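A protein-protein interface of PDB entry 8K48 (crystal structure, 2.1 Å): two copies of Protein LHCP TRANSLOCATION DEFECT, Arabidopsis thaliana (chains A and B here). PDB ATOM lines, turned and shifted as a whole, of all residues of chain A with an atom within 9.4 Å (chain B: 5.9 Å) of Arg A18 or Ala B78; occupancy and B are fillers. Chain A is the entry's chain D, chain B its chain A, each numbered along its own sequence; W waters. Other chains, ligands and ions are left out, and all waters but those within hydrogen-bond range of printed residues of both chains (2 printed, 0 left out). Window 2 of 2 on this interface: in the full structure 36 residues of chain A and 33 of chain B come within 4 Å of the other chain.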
ATOM      1  N   SER A  15     -12.251  -0.458   7.904  1.00  0.00           N
ATOM      2  CA  SER A  15     -11.186   0.494   7.592  1.00  0.00           C
ATOM      3  C   SER A  15     -11.181   1.634   8.606  1.00  0.00           C
ATOM      4  O   SER A  15     -12.055   1.709   9.479  1.00  0.00           O
ATOM      5  CB  SER A  15     -11.353   1.054   6.180  1.00  0.00           C
ATOM      6  OG  SER A  15     -12.646   1.608   6.006  1.00  0.00           O
ATOM      7  N   GLN A  16     -10.196   2.525   8.489  1.00  0.00           N
ATOM      8  CA  GLN A  16     -10.058   3.631   9.421  1.00  0.00           C
ATOM      9  C   GLN A  16     -10.008   4.951   8.673  1.00  0.00           C
ATOM     10  O   GLN A  16      -9.627   5.016   7.500  1.00  0.00           O
ATOM     11  CB  GLN A  16      -8.808   3.480  10.301  1.00  0.00           C
ATOM     12  CG  GLN A  16      -9.091   2.871  11.661  1.00  0.00           C
ATOM     13  CD  GLN A  16      -7.824   2.530  12.420  1.00  0.00           C
ATOM     14  OE1 GLN A  16      -6.838   2.073  11.835  1.00  0.00           O
ATOM     15  NE2 GLN A  16      -7.841   2.752  13.726  1.00  0.00           N
ATOM     16  N   SER A  17     -10.267   6.046   9.403  1.00  0.00           N
ATOM     17  CA  SER A  17     -10.216   7.406   8.798  1.00  0.00           C
ATOM     18  C   SER A  17      -9.215   8.316   9.527  1.00  0.00           C
ATOM     19  O   SER A  17      -8.750   7.933  10.612  1.00  0.00           O
ATOM     20  CB  SER A  17     -11.578   8.035   8.789  1.00  0.00           C
ATOM     21  OG  SER A  17     -11.526   9.343   8.240  1.00  0.00           O
ATOM     22  N   ARG A  18      -8.931   9.496   8.964  1.00  0.00           N
ATOM     23  CA  ARG A  18      -7.938  10.437   9.550  1.00  0.00           C
ATOM     24  C   ARG A  18      -8.400  10.900  10.930  1.00  0.00           C
ATOM     25  O   ARG A  18      -7.561  10.982  11.837  1.00  0.00           O
ATOM     26  CB  ARG A  18      -7.770  11.663   8.647  1.00  0.00           C
ATOM     27  CG  ARG A  18      -6.790  11.477   7.501  1.00  0.00           C
ATOM     28  CD  ARG A  18      -6.750  12.726   6.643  1.00  0.00           C
ATOM     29  NE  ARG A  18      -6.322  13.898   7.393  1.00  0.00           N
ATOM     30  CZ  ARG A  18      -5.053  14.232   7.599  1.00  0.00           C
ATOM     31  NH1 ARG A  18      -4.087  13.537   7.029  1.00  0.00           N
ATOM     32  NH2 ARG A  18      -4.756  15.262   8.371  1.00  0.00           N
ATOM     33  N   ASP A  19      -9.695  11.170  11.076  1.00  0.00           N
ATOM     34  CA  ASP A  19     -10.209  11.707  12.361  1.00  0.00           C
ATOM     35  C   ASP A  19     -10.346  10.584  13.390  1.00  0.00           C
ATOM     36  O   ASP A  19     -10.782  10.888  14.509  1.00  0.00           O
ATOM     37  CB  ASP A  19     -11.493  12.510  12.142  1.00  0.00           C
ATOM     38  CG  ASP A  19     -11.338  13.542  11.040  1.00  0.00           C
ATOM     39  OD1 ASP A  19     -10.803  14.632  11.328  1.00  0.00           O
ATOM     40  OD2 ASP A  19     -11.735  13.240   9.899  1.00  0.00           O
ATOM     41  N   ASP A  20      -9.978   9.349  13.043  1.00  0.00           N
ATOM     42  CA  ASP A  20      -9.987   8.313  14.073  1.00  0.00           C
ATOM     43  C   ASP A  20      -8.746   8.356  14.975  1.00  0.00           C
ATOM     44  O   ASP A  20      -8.551   7.449  15.797  1.00  0.00           O
ATOM     45  CB  ASP A  20     -10.107   6.929  13.424  1.00  0.00           C
ATOM     46  CG  ASP A  20     -11.517   6.633  12.917  1.00  0.00           C
ATOM     47  OD1 ASP A  20     -12.484   7.279  13.392  1.00  0.00           O
ATOM     48  OD2 ASP A  20     -11.652   5.759  12.033  1.00  0.00           O
ATOM     49  N   PHE A  21      -7.914   9.386  14.844  1.00  0.00           N
ATOM     50  CA  PHE A  21      -6.654   9.488  15.567  1.00  0.00           C
ATOM     51  C   PHE A  21      -6.626  10.796  16.338  1.00  0.00           C
ATOM     52  O   PHE A  21      -6.811  11.862  15.745  1.00  0.00           O
ATOM     53  CB  PHE A  21      -5.479   9.393  14.595  1.00  0.00           C
ATOM     54  CG  PHE A  21      -5.415   8.077  13.888  1.00  0.00           C
ATOM     55  CD1 PHE A  21      -4.824   6.979  14.500  1.00  0.00           C
ATOM     56  CD2 PHE A  21      -5.983   7.918  12.637  1.00  0.00           C
ATOM     57  CE1 PHE A  21      -4.776   5.757  13.868  1.00  0.00           C
ATOM     58  CE2 PHE A  21      -5.939   6.700  12.003  1.00  0.00           C
ATOM     59  CZ  PHE A  21      -5.336   5.618  12.616  1.00  0.00           C
ATOM     60  N   ASP A  22      -6.392  10.717  17.646  1.00  0.00           N
ATOM     61  CA  ASP A  22      -6.500  11.879  18.523  1.00  0.00           C
ATOM     62  C   ASP A  22      -5.192  12.121  19.283  1.00  0.00           C
ATOM     63  O   ASP A  22      -4.213  11.386  19.151  1.00  0.00           O
ATOM     64  CB  ASP A  22      -7.688  11.724  19.490  1.00  0.00           C
ATOM     65  CG  ASP A  22      -7.583  10.492  20.390  1.00  0.00           C
ATOM     66  OD1 ASP A  22      -6.546   9.803  20.377  1.00  0.00           O
ATOM     67  OD2 ASP A  22      -8.555  10.200  21.123  1.00  0.00           O
ATOM     68  N   ARG A  23      -5.196  13.183  20.090  1.00  0.00           N
ATOM     69  CA  ARG A  23      -4.033  13.534  20.901  1.00  0.00           C
ATOM     70  C   ARG A  23      -3.565  12.366  21.746  1.00  0.00           C
ATOM     71  O   ARG A  23      -2.362  12.091  21.827  1.00  0.00           O
ATOM     72  CB  ARG A  23      -4.367  14.729  21.797  1.00  0.00           C
ATOM     73  CG  ARG A  23      -3.244  15.129  22.737  1.00  0.00           C
ATOM     74  CD  ARG A  23      -3.719  16.125  23.792  1.00  0.00           C
ATOM     75  NE  ARG A  23      -2.779  17.230  23.959  1.00  0.00           N
ATOM     76  CZ  ARG A  23      -2.704  18.286  23.146  1.00  0.00           C
ATOM     77  NH1 ARG A  23      -3.512  18.393  22.091  1.00  0.00           N
ATOM     78  NH2 ARG A  23      -1.813  19.245  23.385  1.00  0.00           N
ATOM     79  N   ASP A  25      -3.777   9.254  21.124  1.00  0.00           N
ATOM     80  CA  ASP A  25      -3.044   8.321  20.260  1.00  0.00           C
ATOM     81  C   ASP A  25      -1.588   8.747  20.096  1.00  0.00           C
ATOM     82  O   ASP A  25      -0.679   7.907  20.155  1.00  0.00           O
ATOM     83  CB  ASP A  25      -3.722   8.218  18.886  1.00  0.00           C
ATOM     84  CG  ASP A  25      -5.054   7.468  18.938  1.00  0.00           C
ATOM     85  OD1 ASP A  25      -5.183   6.540  19.764  1.00  0.00           O
ATOM     86  OD2 ASP A  25      -5.950   7.806  18.140  1.00  0.00           O
ATOM     87  N   HIS B  54      -2.648  17.655  12.515  1.00  0.00           N
ATOM     88  CA  HIS B  54      -3.587  16.572  12.894  1.00  0.00           C
ATOM     89  C   HIS B  54      -2.796  15.420  13.518  1.00  0.00           C
ATOM     90  O   HIS B  54      -1.705  15.078  13.040  1.00  0.00           O
ATOM     91  CB  HIS B  54      -4.426  16.116  11.700  1.00  0.00           C
ATOM     92  CG  HIS B  54      -5.354  17.155  11.168  1.00  0.00           C
ATOM     93  ND1 HIS B  54      -4.939  18.218  10.397  1.00  0.00           N
ATOM     94  CD2 HIS B  54      -6.682  17.264  11.264  1.00  0.00           C
ATOM     95  CE1 HIS B  54      -5.989  18.952  10.066  1.00  0.00           C
ATOM     96  NE2 HIS B  54      -7.057  18.393  10.586  1.00  0.00           N
ATOM     97  N   VAL B  56      -3.105  12.304  13.192  1.00  0.00           N
ATOM     98  CA  VAL B  56      -2.771  11.200  12.298  1.00  0.00           C
ATOM     99  C   VAL B  56      -1.491  11.506  11.516  1.00  0.00           C
ATOM    100  O   VAL B  56      -0.673  10.608  11.277  1.00  0.00           O
ATOM    101  CB  VAL B  56      -3.962  10.879  11.372  1.00  0.00           C
ATOM    102  CG1 VAL B  56      -4.297  12.079  10.496  1.00  0.00           C
ATOM    103  CG2 VAL B  56      -3.660   9.651  10.525  1.00  0.00           C
ATOM    104  N   ASP B  57      -1.289  12.773  11.121  1.00  0.00           N
ATOM    105  CA  ASP B  57      -0.046  13.151  10.453  1.00  0.00           C
ATOM    106  C   ASP B  57       1.130  13.137  11.422  1.00  0.00           C
ATOM    107  O   ASP B  57       2.258  12.815  11.025  1.00  0.00           O
ATOM    108  CB  ASP B  57      -0.168  14.544   9.831  1.00  0.00           C
ATOM    109  CG  ASP B  57      -1.301  14.646   8.809  1.00  0.00           C
ATOM    110  OD1 ASP B  57      -1.608  13.636   8.125  1.00  0.00           O
ATOM    111  OD2 ASP B  57      -1.874  15.756   8.692  1.00  0.00           O
ATOM    112  N   GLU B  73       1.941   1.736   7.370  1.00  0.00           N
ATOM    113  CA  GLU B  73       0.900   1.249   6.475  1.00  0.00           C
ATOM    114  C   GLU B  73      -0.486   1.553   7.028  1.00  0.00           C
ATOM    115  O   GLU B  73      -1.370   2.008   6.294  1.00  0.00           O
ATOM    116  CB  GLU B  73       1.088  -0.250   6.240  1.00  0.00           C
ATOM    117  CG  GLU B  73       2.476  -0.609   5.728  1.00  0.00           C
ATOM    118  CD  GLU B  73       2.509  -1.935   4.994  1.00  0.00           C
ATOM    119  OE1 GLU B  73       2.744  -1.923   3.763  1.00  0.00           O
ATOM    120  OE2 GLU B  73       2.309  -2.987   5.646  1.00  0.00           O
ATOM    121  N   GLU B  74      -0.694   1.323   8.324  1.00  0.00           N
ATOM    122  CA  GLU B  74      -1.987   1.635   8.921  1.00  0.00           C
ATOM    123  C   GLU B  74      -2.329   3.108   8.758  1.00  0.00           C
ATOM    124  O   GLU B  74      -3.471   3.459   8.427  1.00  0.00           O
ATOM    125  CB  GLU B  74      -1.998   1.260  10.401  1.00  0.00           C
ATOM    126  CG  GLU B  74      -3.257   1.731  11.110  1.00  0.00           C
ATOM    127  CD  GLU B  74      -3.113   1.804  12.619  1.00  0.00           C
ATOM    128  OE1 GLU B  74      -4.150   1.975  13.297  1.00  0.00           O
ATOM    129  OE2 GLU B  74      -1.978   1.696  13.127  1.00  0.00           O
ATOM    130  N   LEU B  75      -1.354   3.990   8.983  1.00  0.00           N
ATOM    131  CA  LEU B  75      -1.659   5.418   8.985  1.00  0.00           C
ATOM    132  C   LEU B  75      -1.936   5.920   7.575  1.00  0.00           C
ATOM    133  O   LEU B  75      -2.827   6.751   7.365  1.00  0.00           O
ATOM    134  CB  LEU B  75      -0.510   6.199   9.625  1.00  0.00           C
ATOM    135  CG  LEU B  75      -0.391   5.986  11.132  1.00  0.00           C
ATOM    136  CD1 LEU B  75       0.985   6.440  11.645  1.00  0.00           C
ATOM    137  CD2 LEU B  75      -1.529   6.680  11.871  1.00  0.00           C
ATOM    138  N   LEU B  76      -1.184   5.426   6.597  1.00  0.00           N
ATOM    139  CA  LEU B  76      -1.435   5.813   5.217  1.00  0.00           C
ATOM    140  C   LEU B  76      -2.819   5.367   4.760  1.00  0.00           C
ATOM    141  O   LEU B  76      -3.555   6.148   4.143  1.00  0.00           O
ATOM    142  CB  LEU B  76      -0.345   5.232   4.324  1.00  0.00           C
ATOM    143  CG  LEU B  76       0.981   5.954   4.539  1.00  0.00           C
ATOM    144  CD1 LEU B  76       2.107   5.237   3.840  1.00  0.00           C
ATOM    145  CD2 LEU B  76       0.860   7.398   4.051  1.00  0.00           C
ATOM    146  N   LYS B  77      -3.199   4.124   5.080  1.00  0.00           N
ATOM    147  CA  LYS B  77      -4.525   3.636   4.717  1.00  0.00           C
ATOM    148  C   LYS B  77      -5.618   4.521   5.288  1.00  0.00           C
ATOM    149  O   LYS B  77      -6.686   4.657   4.682  1.00  0.00           O
ATOM    150  CB  LYS B  77      -4.719   2.200   5.201  1.00  0.00           C
ATOM    151  CG  LYS B  77      -4.470   1.139   4.143  1.00  0.00           C
ATOM    152  CD  LYS B  77      -4.684  -0.269   4.698  1.00  0.00           C
ATOM    153  CE  LYS B  77      -3.746  -1.294   4.044  1.00  0.00           C
ATOM    154  NZ  LYS B  77      -4.461  -2.369   3.273  1.00  0.00           N
ATOM    155  N   ALA B  78      -5.376   5.134   6.445  1.00  0.00           N
ATOM    156  CA  ALA B  78      -6.359   6.030   7.037  1.00  0.00           C
ATOM    157  C   ALA B  78      -6.274   7.442   6.480  1.00  0.00           C
ATOM    158  O   ALA B  78      -7.075   8.294   6.873  1.00  0.00           O
ATOM    159  CB  ALA B  78      -6.201   6.061   8.558  1.00  0.00           C
ATOM    160  N   GLY B  79      -5.324   7.710   5.592  1.00  0.00           N
ATOM    161  CA  GLY B  79      -5.214   9.003   4.956  1.00  0.00           C
ATOM    162  C   GLY B  79      -4.161   9.941   5.506  1.00  0.00           C
ATOM    163  O   GLY B  79      -4.314  11.157   5.355  1.00  0.00           O
ATOM    164  N   ALA B  80      -3.095   9.423   6.118  1.00  0.00           N
ATOM    165  CA  ALA B  80      -2.024  10.284   6.607  1.00  0.00           C
ATOM    166  C   ALA B  80      -1.313  10.987   5.452  1.00  0.00           C
ATOM    167  O   ALA B  80      -1.020  10.381   4.415  1.00  0.00           O
ATOM    168  CB  ALA B  80      -1.021   9.461   7.418  1.00  0.00           C
ATOM    169  N   ASP B  81      -1.025  12.275   5.646  1.00  0.00           N
ATOM    170  CA  ASP B  81      -0.374  13.121   4.648  1.00  0.00           C
ATOM    171  C   ASP B  81       1.114  13.220   4.976  1.00  0.00           C
ATOM    172  O   ASP B  81       1.482  13.703   6.051  1.00  0.00           O
ATOM    173  CB  ASP B  81      -1.033  14.506   4.633  1.00  0.00           C
ATOM    174  CG  ASP B  81      -0.424  15.464   3.607  1.00  0.00           C
ATOM    175  OD1 ASP B  81       0.685  15.222   3.084  1.00  0.00           O
ATOM    176  OD2 ASP B  81      -1.061  16.510   3.350  1.00  0.00           O
HETATM  177  O   HOH W   1      -5.879   1.992   9.108  1.00  0.00           O
HETATM  178  O   HOH W   2      -8.599  15.907   9.270  1.00  0.00           O
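No position is printed for both chains.
Of the 14 pairs that touch across the chains among the printed residues, none has its exchanged pair printed and touching as well.
Of the printed residues of chain B, Arg A18 touches His B54 (3.4 Å), Val B56 (3.6 Å), Asp B57 (2.7 Å), Ala B78 (3.0 Å), Gly B79 (2.9 Å), Ala B80 (3.9 Å) and Asp B81 (3.6 Å).
Of the printed residues of chain B, Phe A21 touches Val B56, Glu B74, Leu B75 and Ala B78.
Of the printed residues of chain A, Glu B74 touches Gln A16 (3.1 Å) and Phe A21 (3.9 Å).
Leu B76 touches none of the printed residues of chain A.
Lys B77 touches none of the printed residues of chain A.
Ala B78 touches just these residues of chain A: Gln A16 (3.5 Å), Ser A17 (3.4 Å), Arg A18 (3.0 Å) and Phe A21 (3.5 Å).
Ala B80 touches just one residue of chain A: Arg A18.
The nearest printed residue of chain B that does not touch Arg A18 is Leu B75 (6.2 Å).
The nearest residue of chain A that does not touch Ala B78 is Asp A19 (5.7 Å).
The nearest printed residue of chain B that does not touch Gln A16 is Lys B77 (4.1 Å).
Water W1 bridges the side-chain amide oxygen (OE1) of Gln A16 (2.9 Å) and the backbone carbonyl oxygen (O) of Glu B74 (2.9 Å).
Water W2 lies within hydrogen-bond range of a ring nitrogen (NE2) of His B54 and the side-chain carboxylate of Asp A19.
N of Arg A18 lies within hydrogen-bond range of O of Ala B78 (3.0 Å).
The backbone carbonyl oxygen (O) of Gly B79 lies within hydrogen-bond range of the guanidinium group (NH1) of Arg A18, at 2.9 Å.
NH1 of Arg A18 is in salt-bridge range of OD1 of Asp B57.
OE1 of Glu B74 lies close to OE1 of Gln A16 (3.1 Å).
The backbone carbonyl oxygen of Leu B75 is in hydrogen-bond range of the backbone NH of Ala B80 (3.0 Å).
OD1 of Asp B57 lies within hydrogen-bond range of N of Asp B81, at 2.9 Å.
The side-chain carboxylate (OD2) of Asp A20 is in hydrogen-bond range of the backbone NH (N) of Ser A17, at 3.0 Å.
Along chain A the printed residues that touch a printed residue of chain B span positions 16 to 21.
Of the 12 printed residues of chain B, 9 touch a printed residue of chain A.
Hydrophobic or aromatic side chains of chain B that line the printed part of chain A: His B54, Val B56, Leu B75 and Ala B78.
Along chain B the printed residues that touch a printed residue of chain A span positions 54 to 81.
Among the printed residues, Asp or Glu carboxylates within 4 Å of a Lys or Arg side-chain nitrogen of the other chain: Arg A18 with Asp B57.
Among the printed residues, merely in contact across the chains: Ser A17 with Ala B78 (3.4 Å), Arg A18 with His B54 (3.4 Å), Gln A16 with Ala B78 (3.5 Å), Phe A21 with Ala B78 (3.5 Å), Phe A21 with Val B56 (3.6 Å), Arg A18 with Asp B81 (3.6 Å), Arg A18 with Val B56 (3.6 Å), Arg A18 with Ala B80 (3.9 Å), Phe A21 with Glu B74 (3.9 Å) and Phe A21 with Leu B75 (3.9 Å).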
